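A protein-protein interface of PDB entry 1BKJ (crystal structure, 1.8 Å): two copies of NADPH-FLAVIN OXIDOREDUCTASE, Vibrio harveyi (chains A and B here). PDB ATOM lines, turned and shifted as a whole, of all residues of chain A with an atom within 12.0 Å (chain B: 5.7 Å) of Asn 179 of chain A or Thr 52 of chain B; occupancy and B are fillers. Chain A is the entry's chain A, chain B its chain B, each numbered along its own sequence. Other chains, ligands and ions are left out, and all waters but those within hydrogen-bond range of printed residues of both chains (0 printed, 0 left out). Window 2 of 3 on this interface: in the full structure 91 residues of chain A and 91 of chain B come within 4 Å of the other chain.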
ATOM      1  N   ALA A 172      28.444   9.710   1.914  1.00  0.00           N
ATOM      2  CA  ALA A 172      28.535   8.255   1.915  1.00  0.00           C
ATOM      3  C   ALA A 172      28.858   7.646   3.270  1.00  0.00           C
ATOM      4  O   ALA A 172      28.352   6.581   3.579  1.00  0.00           O
ATOM      5  CB  ALA A 172      29.540   7.791   0.879  1.00  0.00           C
ATOM      6  N   HIS A 173      29.640   8.340   4.102  1.00  0.00           N
ATOM      7  CA  HIS A 173      29.976   7.807   5.427  1.00  0.00           C
ATOM      8  C   HIS A 173      28.796   7.796   6.435  1.00  0.00           C
ATOM      9  O   HIS A 173      28.900   7.184   7.504  1.00  0.00           O
ATOM     10  CB  HIS A 173      31.245   8.475   6.001  1.00  0.00           C
ATOM     11  CG  HIS A 173      31.083   9.920   6.360  1.00  0.00           C
ATOM     12  ND1 HIS A 173      31.524  10.940   5.544  1.00  0.00           N
ATOM     13  CD2 HIS A 173      30.556  10.517   7.457  1.00  0.00           C
ATOM     14  CE1 HIS A 173      31.275  12.102   6.123  1.00  0.00           C
ATOM     15  NE2 HIS A 173      30.686  11.871   7.282  1.00  0.00           N
ATOM     16  N   VAL A 174      27.709   8.505   6.096  1.00  0.00           N
ATOM     17  CA  VAL A 174      26.478   8.557   6.906  1.00  0.00           C
ATOM     18  C   VAL A 174      25.527   7.433   6.445  1.00  0.00           C
ATOM     19  O   VAL A 174      25.052   6.640   7.269  1.00  0.00           O
ATOM     20  CB  VAL A 174      25.760   9.952   6.782  1.00  0.00           C
ATOM     21  CG1 VAL A 174      24.382   9.965   7.450  1.00  0.00           C
ATOM     22  CG2 VAL A 174      26.606  11.028   7.406  1.00  0.00           C
ATOM     23  N   VAL A 175      25.292   7.357   5.131  1.00  0.00           N
ATOM     24  CA  VAL A 175      24.384   6.377   4.508  1.00  0.00           C
ATOM     25  C   VAL A 175      24.925   4.938   4.481  1.00  0.00           C
ATOM     26  O   VAL A 175      24.146   3.996   4.671  1.00  0.00           O
ATOM     27  CB  VAL A 175      23.943   6.867   3.075  1.00  0.00           C
ATOM     28  CG1 VAL A 175      23.002   5.863   2.380  1.00  0.00           C
ATOM     29  CG2 VAL A 175      23.240   8.223   3.188  1.00  0.00           C
ATOM     30  N   VAL A 176      26.238   4.781   4.265  1.00  0.00           N
ATOM     31  CA  VAL A 176      26.890   3.464   4.218  1.00  0.00           C
ATOM     32  C   VAL A 176      27.514   3.067   5.566  1.00  0.00           C
ATOM     33  O   VAL A 176      28.300   3.809   6.165  1.00  0.00           O
ATOM     34  CB  VAL A 176      27.948   3.364   3.066  1.00  0.00           C
ATOM     35  CG1 VAL A 176      28.534   1.949   2.946  1.00  0.00           C
ATOM     36  CG2 VAL A 176      27.321   3.764   1.753  1.00  0.00           C
ATOM     37  N   HIS A 177      27.124   1.879   6.016  1.00  0.00           N
ATOM     38  CA  HIS A 177      27.574   1.277   7.263  1.00  0.00           C
ATOM     39  C   HIS A 177      28.403   0.042   6.933  1.00  0.00           C
ATOM     40  O   HIS A 177      28.116  -0.650   5.957  1.00  0.00           O
ATOM     41  CB  HIS A 177      26.367   0.830   8.080  1.00  0.00           C
ATOM     42  CG  HIS A 177      25.396   1.927   8.376  1.00  0.00           C
ATOM     43  ND1 HIS A 177      25.388   2.603   9.577  1.00  0.00           N
ATOM     44  CD2 HIS A 177      24.417   2.481   7.626  1.00  0.00           C
ATOM     45  CE1 HIS A 177      24.453   3.529   9.551  1.00  0.00           C
ATOM     46  NE2 HIS A 177      23.843   3.476   8.376  1.00  0.00           N
ATOM     47  N   GLU A 178      29.435  -0.219   7.736  1.00  0.00           N
ATOM     48  CA  GLU A 178      30.299  -1.392   7.544  1.00  0.00           C
ATOM     49  C   GLU A 178      29.984  -2.462   8.601  1.00  0.00           C
ATOM     50  O   GLU A 178      30.145  -2.223   9.805  1.00  0.00           O
ATOM     51  CB  GLU A 178      31.784  -1.007   7.630  1.00  0.00           C
ATOM     52  CG  GLU A 178      32.255   0.088   6.653  1.00  0.00           C
ATOM     53  CD  GLU A 178      33.020  -0.455   5.448  1.00  0.00           C
ATOM     54  OE1 GLU A 178      33.761  -1.468   5.600  1.00  0.00           O
ATOM     55  OE2 GLU A 178      32.891   0.148   4.352  1.00  0.00           O
ATOM     56  N   ASN A 179      29.464  -3.598   8.132  1.00  0.00           N
ATOM     57  CA  ASN A 179      29.109  -4.784   8.934  1.00  0.00           C
ATOM     58  C   ASN A 179      28.013  -4.713  10.003  1.00  0.00           C
ATOM     59  O   ASN A 179      27.297  -5.697  10.227  1.00  0.00           O
ATOM     60  CB  ASN A 179      30.367  -5.441   9.517  1.00  0.00           C
ATOM     61  CG  ASN A 179      31.262  -6.004   8.449  1.00  0.00           C
ATOM     62  OD1 ASN A 179      30.815  -6.764   7.600  1.00  0.00           O
ATOM     63  ND2 ASN A 179      32.536  -5.642   8.487  1.00  0.00           N
ATOM     64  N   GLN A 180      27.910  -3.573  10.682  1.00  0.00           N
ATOM     65  CA  GLN A 180      26.903  -3.359  11.722  1.00  0.00           C
ATOM     66  C   GLN A 180      26.450  -1.912  11.603  1.00  0.00           C
ATOM     67  O   GLN A 180      27.210  -1.065  11.134  1.00  0.00           O
ATOM     68  CB  GLN A 180      27.502  -3.604  13.122  1.00  0.00           C
ATOM     69  N   TYR A 181      25.209  -1.628  11.996  1.00  0.00           N
ATOM     70  CA  TYR A 181      24.685  -0.262  11.949  1.00  0.00           C
ATOM     71  C   TYR A 181      25.443   0.640  12.945  1.00  0.00           C
ATOM     72  O   TYR A 181      25.589   0.294  14.119  1.00  0.00           O
ATOM     73  CB  TYR A 181      23.174  -0.257  12.246  1.00  0.00           C
ATOM     74  CG  TYR A 181      22.445   1.055  11.971  1.00  0.00           C
ATOM     75  CD1 TYR A 181      22.404   2.095  12.944  1.00  0.00           C
ATOM     76  CD2 TYR A 181      21.752   1.256  10.753  1.00  0.00           C
ATOM     77  CE1 TYR A 181      21.681   3.309  12.717  1.00  0.00           C
ATOM     78  CE2 TYR A 181      21.019   2.464  10.511  1.00  0.00           C
ATOM     79  CZ  TYR A 181      20.993   3.487  11.499  1.00  0.00           C
ATOM     80  OH  TYR A 181      20.295   4.657  11.276  1.00  0.00           O
ATOM     81  N   GLN A 182      25.904   1.790  12.446  1.00  0.00           N
ATOM     82  CA  GLN A 182      26.652   2.792  13.220  1.00  0.00           C
ATOM     83  C   GLN A 182      25.726   3.918  13.687  1.00  0.00           C
ATOM     84  O   GLN A 182      24.915   4.408  12.902  1.00  0.00           O
ATOM     85  CB  GLN A 182      27.783   3.388  12.360  1.00  0.00           C
ATOM     86  N   GLU A 183      25.838   4.317  14.958  1.00  0.00           N
ATOM     87  CA  GLU A 183      25.025   5.409  15.521  1.00  0.00           C
ATOM     88  C   GLU A 183      25.355   6.735  14.802  1.00  0.00           C
ATOM     89  O   GLU A 183      26.490   6.931  14.324  1.00  0.00           O
ATOM     90  CB  GLU A 183      25.270   5.546  17.034  1.00  0.00           C
ATOM     91  N   VAL B  49      24.175  -1.355   4.196  1.00  0.00           N
ATOM     92  CA  VAL B  49      25.122  -2.031   5.078  1.00  0.00           C
ATOM     93  C   VAL B  49      26.051  -2.877   4.201  1.00  0.00           C
ATOM     94  O   VAL B  49      25.602  -3.804   3.529  1.00  0.00           O
ATOM     95  CB  VAL B  49      24.431  -2.917   6.159  1.00  0.00           C
ATOM     96  CG1 VAL B  49      25.480  -3.568   7.069  1.00  0.00           C
ATOM     97  CG2 VAL B  49      23.480  -2.083   7.013  1.00  0.00           C
ATOM     98  N   ARG B  50      27.327  -2.509   4.165  1.00  0.00           N
ATOM     99  CA  ARG B  50      28.336  -3.240   3.402  1.00  0.00           C
ATOM    100  C   ARG B  50      28.841  -4.378   4.304  1.00  0.00           C
ATOM    101  O   ARG B  50      29.258  -4.125   5.429  1.00  0.00           O
ATOM    102  CB  ARG B  50      29.479  -2.296   3.029  1.00  0.00           C
ATOM    103  CG  ARG B  50      30.546  -2.943   2.166  1.00  0.00           C
ATOM    104  CD  ARG B  50      31.778  -2.075   2.049  1.00  0.00           C
ATOM    105  NE  ARG B  50      32.833  -2.751   1.292  1.00  0.00           N
ATOM    106  CZ  ARG B  50      34.141  -2.563   1.459  1.00  0.00           C
ATOM    107  NH1 ARG B  50      34.595  -1.715   2.372  1.00  0.00           N
ATOM    108  NH2 ARG B  50      34.996  -3.203   0.675  1.00  0.00           N
ATOM    109  N   VAL B  51      28.741  -5.626   3.845  1.00  0.00           N
ATOM    110  CA  VAL B  51      29.188  -6.775   4.647  1.00  0.00           C
ATOM    111  C   VAL B  51      30.527  -7.327   4.159  1.00  0.00           C
ATOM    112  O   VAL B  51      30.588  -8.025   3.148  1.00  0.00           O
ATOM    113  CB  VAL B  51      28.112  -7.906   4.695  1.00  0.00           C
ATOM    114  CG1 VAL B  51      28.544  -9.042   5.624  1.00  0.00           C
ATOM    115  CG2 VAL B  51      26.789  -7.347   5.178  1.00  0.00           C
ATOM    116  N   THR B  52      31.587  -7.012   4.902  1.00  0.00           N
ATOM    117  CA  THR B  52      32.941  -7.459   4.583  1.00  0.00           C
ATOM    118  C   THR B  52      33.408  -8.641   5.434  1.00  0.00           C
ATOM    119  O   THR B  52      34.365  -9.332   5.077  1.00  0.00           O
ATOM    120  CB  THR B  52      33.948  -6.317   4.723  1.00  0.00           C
ATOM    121  OG1 THR B  52      33.840  -5.738   6.026  1.00  0.00           O
ATOM    122  CG2 THR B  52      33.690  -5.267   3.674  1.00  0.00           C
ATOM    123  N   ASP B  53      32.740  -8.833   6.569  1.00  0.00           N
ATOM    124  CA  ASP B  53      32.997  -9.910   7.535  1.00  0.00           C
ATOM    125  C   ASP B  53      32.575 -11.230   6.863  1.00  0.00           C
ATOM    126  O   ASP B  53      31.401 -11.405   6.527  1.00  0.00           O
ATOM    127  CB  ASP B  53      32.145  -9.615   8.790  1.00  0.00           C
ATOM    128  CG  ASP B  53      32.399 -10.563   9.971  1.00  0.00           C
ATOM    129  OD1 ASP B  53      32.580 -11.785   9.779  1.00  0.00           O
ATOM    130  OD2 ASP B  53      32.331 -10.075  11.123  1.00  0.00           O
ATOM    131  N   SER B  54      33.538 -12.138   6.672  1.00  0.00           N
ATOM    132  CA  SER B  54      33.295 -13.439   6.026  1.00  0.00           C
ATOM    133  C   SER B  54      32.395 -14.415   6.806  1.00  0.00           C
ATOM    134  O   SER B  54      31.703 -15.229   6.187  1.00  0.00           O
ATOM    135  CB  SER B  54      34.625 -14.108   5.632  1.00  0.00           C
ATOM    136  OG  SER B  54      35.436 -14.397   6.766  1.00  0.00           O
ATOM    137  N   LYS B  56      29.885 -13.376   8.799  1.00  0.00           N
ATOM    138  CA  LYS B  56      28.541 -12.812   8.620  1.00  0.00           C
ATOM    139  C   LYS B  56      27.992 -13.167   7.238  1.00  0.00           C
ATOM    140  O   LYS B  56      26.822 -13.512   7.137  1.00  0.00           O
ATOM    141  CB  LYS B  56      28.509 -11.295   8.835  1.00  0.00           C
ATOM    142  CG  LYS B  56      28.494 -10.892  10.304  1.00  0.00           C
ATOM    143  CD  LYS B  56      28.083  -9.437  10.500  1.00  0.00           C
ATOM    144  CE  LYS B  56      28.196  -9.028  11.976  1.00  0.00           C
ATOM    145  NZ  LYS B  56      27.696  -7.642  12.239  1.00  0.00           N
ATOM    146  N   ARG B  57      28.855 -13.162   6.208  1.00  0.00           N
ATOM    147  CA  ARG B  57      28.487 -13.518   4.824  1.00  0.00           C
ATOM    148  C   ARG B  57      27.968 -14.948   4.743  1.00  0.00           C
ATOM    149  O   ARG B  57      26.959 -15.187   4.080  1.00  0.00           O
ATOM    150  CB  ARG B  57      29.678 -13.417   3.873  1.00  0.00           C
ATOM    151  CG  ARG B  57      30.115 -12.027   3.505  1.00  0.00           C
ATOM    152  CD  ARG B  57      29.370 -11.474   2.304  1.00  0.00           C
ATOM    153  NE  ARG B  57      30.201 -10.455   1.668  1.00  0.00           N
ATOM    154  CZ  ARG B  57      30.760 -10.573   0.463  1.00  0.00           C
ATOM    155  NH1 ARG B  57      30.559 -11.658  -0.272  1.00  0.00           N
ATOM    156  NH2 ARG B  57      31.612  -9.648   0.036  1.00  0.00           N
ATOM    157  N   GLU B  75      31.423  -8.010  -3.360  1.00  0.00           N
ATOM    158  CA  GLU B  75      30.720  -7.077  -2.474  1.00  0.00           C
ATOM    159  C   GLU B  75      29.274  -7.507  -2.272  1.00  0.00           C
ATOM    160  O   GLU B  75      28.636  -8.026  -3.192  1.00  0.00           O
ATOM    161  CB  GLU B  75      30.734  -5.637  -3.027  1.00  0.00           C
ATOM    162  CG  GLU B  75      32.102  -4.923  -3.111  1.00  0.00           C
ATOM    163  CD  GLU B  75      32.775  -4.695  -1.766  1.00  0.00           C
ATOM    164  OE1 GLU B  75      32.068  -4.391  -0.786  1.00  0.00           O
ATOM    165  OE2 GLU B  75      34.021  -4.797  -1.691  1.00  0.00           O
ATOM    166  N   LEU B 142      21.489  -9.620  13.295  1.00  0.00           N
ATOM    167  CA  LEU B 142      22.885  -9.813  12.875  1.00  0.00           C
ATOM    168  C   LEU B 142      23.556  -8.515  12.433  1.00  0.00           C
ATOM    169  O   LEU B 142      24.734  -8.291  12.736  1.00  0.00           O
ATOM    170  CB  LEU B 142      22.979 -10.847  11.742  1.00  0.00           C
ATOM    171  CG  LEU B 142      24.343 -11.326  11.224  1.00  0.00           C
ATOM    172  CD1 LEU B 142      25.090 -12.107  12.293  1.00  0.00           C
ATOM    173  CD2 LEU B 142      24.151 -12.200  10.011  1.00  0.00           C
ATOM    174  N   LEU B 143      22.804  -7.663  11.733  1.00  0.00           N
ATOM    175  CA  LEU B 143      23.330  -6.389  11.251  1.00  0.00           C
ATOM    176  C   LEU B 143      23.165  -5.257  12.265  1.00  0.00           C
ATOM    177  O   LEU B 143      23.609  -4.132  12.012  1.00  0.00           O
ATOM    178  CB  LEU B 143      22.689  -6.005   9.906  1.00  0.00           C
ATOM    179  CG  LEU B 143      22.801  -6.963   8.713  1.00  0.00           C
ATOM    180  CD1 LEU B 143      22.036  -6.366   7.551  1.00  0.00           C
ATOM    181  CD2 LEU B 143      24.258  -7.233   8.321  1.00  0.00           C
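The backbone carbonyl oxygen of His 177 of chain A is in hydrogen-bond range of the backbone NH of Arg 50 of chain B (2.7 Å). The backbone NH (N) of Tyr 181 of chain A lies within hydrogen-bond range of the backbone carbonyl oxygen (O) of Leu 143 of chain B. The backbone NH (N) of Asn 179 of chain A is in hydrogen-bond range of the backbone carbonyl oxygen (O) of Arg 50 of chain B (2.8 Å). OG1 of Thr 52 of chain B is in hydrogen-bond range of ND2 of Asn 179 of chain A (2.8 Å). The guanidinium group of Arg 50 of chain B lies within salt-bridge range of the side-chain carboxylate of Glu 178 of chain A, 3.2 Å away. The side-chain amide oxygen (OD1) of Asn 179 of chain A lies within hydrogen-bond range of the backbone NH (N) of Asp 53 of chain B, 3.0 Å away. The backbone carbonyl oxygen (O) of Asn 179 of chain A sits at hydrogen-bond distance from the side-chain amino group (NZ) of Lys 56 of chain B (2.8 Å).
No position is printed for both chains.
The backbone NH (N) of Lys 56 of chain B is in hydrogen-bond range of the side-chain carboxylate (OD1) of Asp 53 of chain B. The side-chain carboxylate (OE1) of Glu 75 of chain B lies within salt-bridge range of the guanidinium group (NE) of Arg 50 of chain B (2.8 Å). The backbone carbonyl oxygen (O) of Val 51 of chain B lies within hydrogen-bond range of the guanidinium group (NE) of Arg 57 of chain B. The backbone carbonyl oxygen (O) of Leu 142 of chain B lies within hydrogen-bond range of the side-chain amino group (NZ) of Lys 56 of chain B, at 3.1 Å. A ring nitrogen (ND1) of His 177 of chain A lies within hydrogen-bond range of the backbone NH (N) of Gln 182 of chain A (3.0 Å).
Among the printed residues, pairs that only touch across the chains: Asn 179 of chain A with Val 51 of chain B (3.4 Å), Gln 180 of chain A with Leu 143 of chain B (3.4 Å), His 177 of chain A with Val 49 of chain B (3.4 Å) and Asn 179 of chain A with Leu 143 of chain B (3.9 Å).
Of the 11 printed residues of chain B, 7 touch a printed residue of chain A. Printed residues of chain B that touch a printed residue of chain A: Val 49, Arg 50, Val 51, Thr 52, Asp 53, Lys 56 and Leu 143. Hydrophobic or aromatic side chains of chain B that line the printed part of chain A: Val 51 and Leu 143.
Of chain B, only Arg 50, Val 51, Thr 52, Asp 53, Lys 56 and Leu 143 come within 4 Å of Asn 179 of chain A. Thr 52 of chain B touches just one residue of chain A: Asn 179 (2.8 Å). Of chain A, only His 177 (3.4 Å) comes within 4 Å of Val 49 of chain B. Arg 50 of chain B touches three residues of chain A. Val 51 of chain B touches one residue of chain A. Of the printed residues of chain A, Asp 53 of chain B touches Asn 179 (3.0 Å). Lys 56 of chain B touches just one residue of chain A: Asn 179. Of the printed residues of chain A, Leu 143 of chain B touches Asn 179, Gln 180 and Tyr 181. Of the printed residues of chain B, Glu 178 of chain A touches Arg 50 (3.2 Å). Of the printed residues of chain B, His 177 of chain A touches Val 49 and Arg 50. Of the printed residues of chain B, Tyr 181 of chain A touches Leu 143. Of the printed residues of chain B, Gln 180 of chain A touches Leu 143. Val 174 of chain A touches none of the printed residues of chain B. The nearest residue of chain B that does not touch Asn 179 of chain A is Val 49 of chain B (4.04 Å). The nearest printed residue of chain B that does not touch Glu 178 of chain A is Thr 52 of chain B (4.3 Å).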
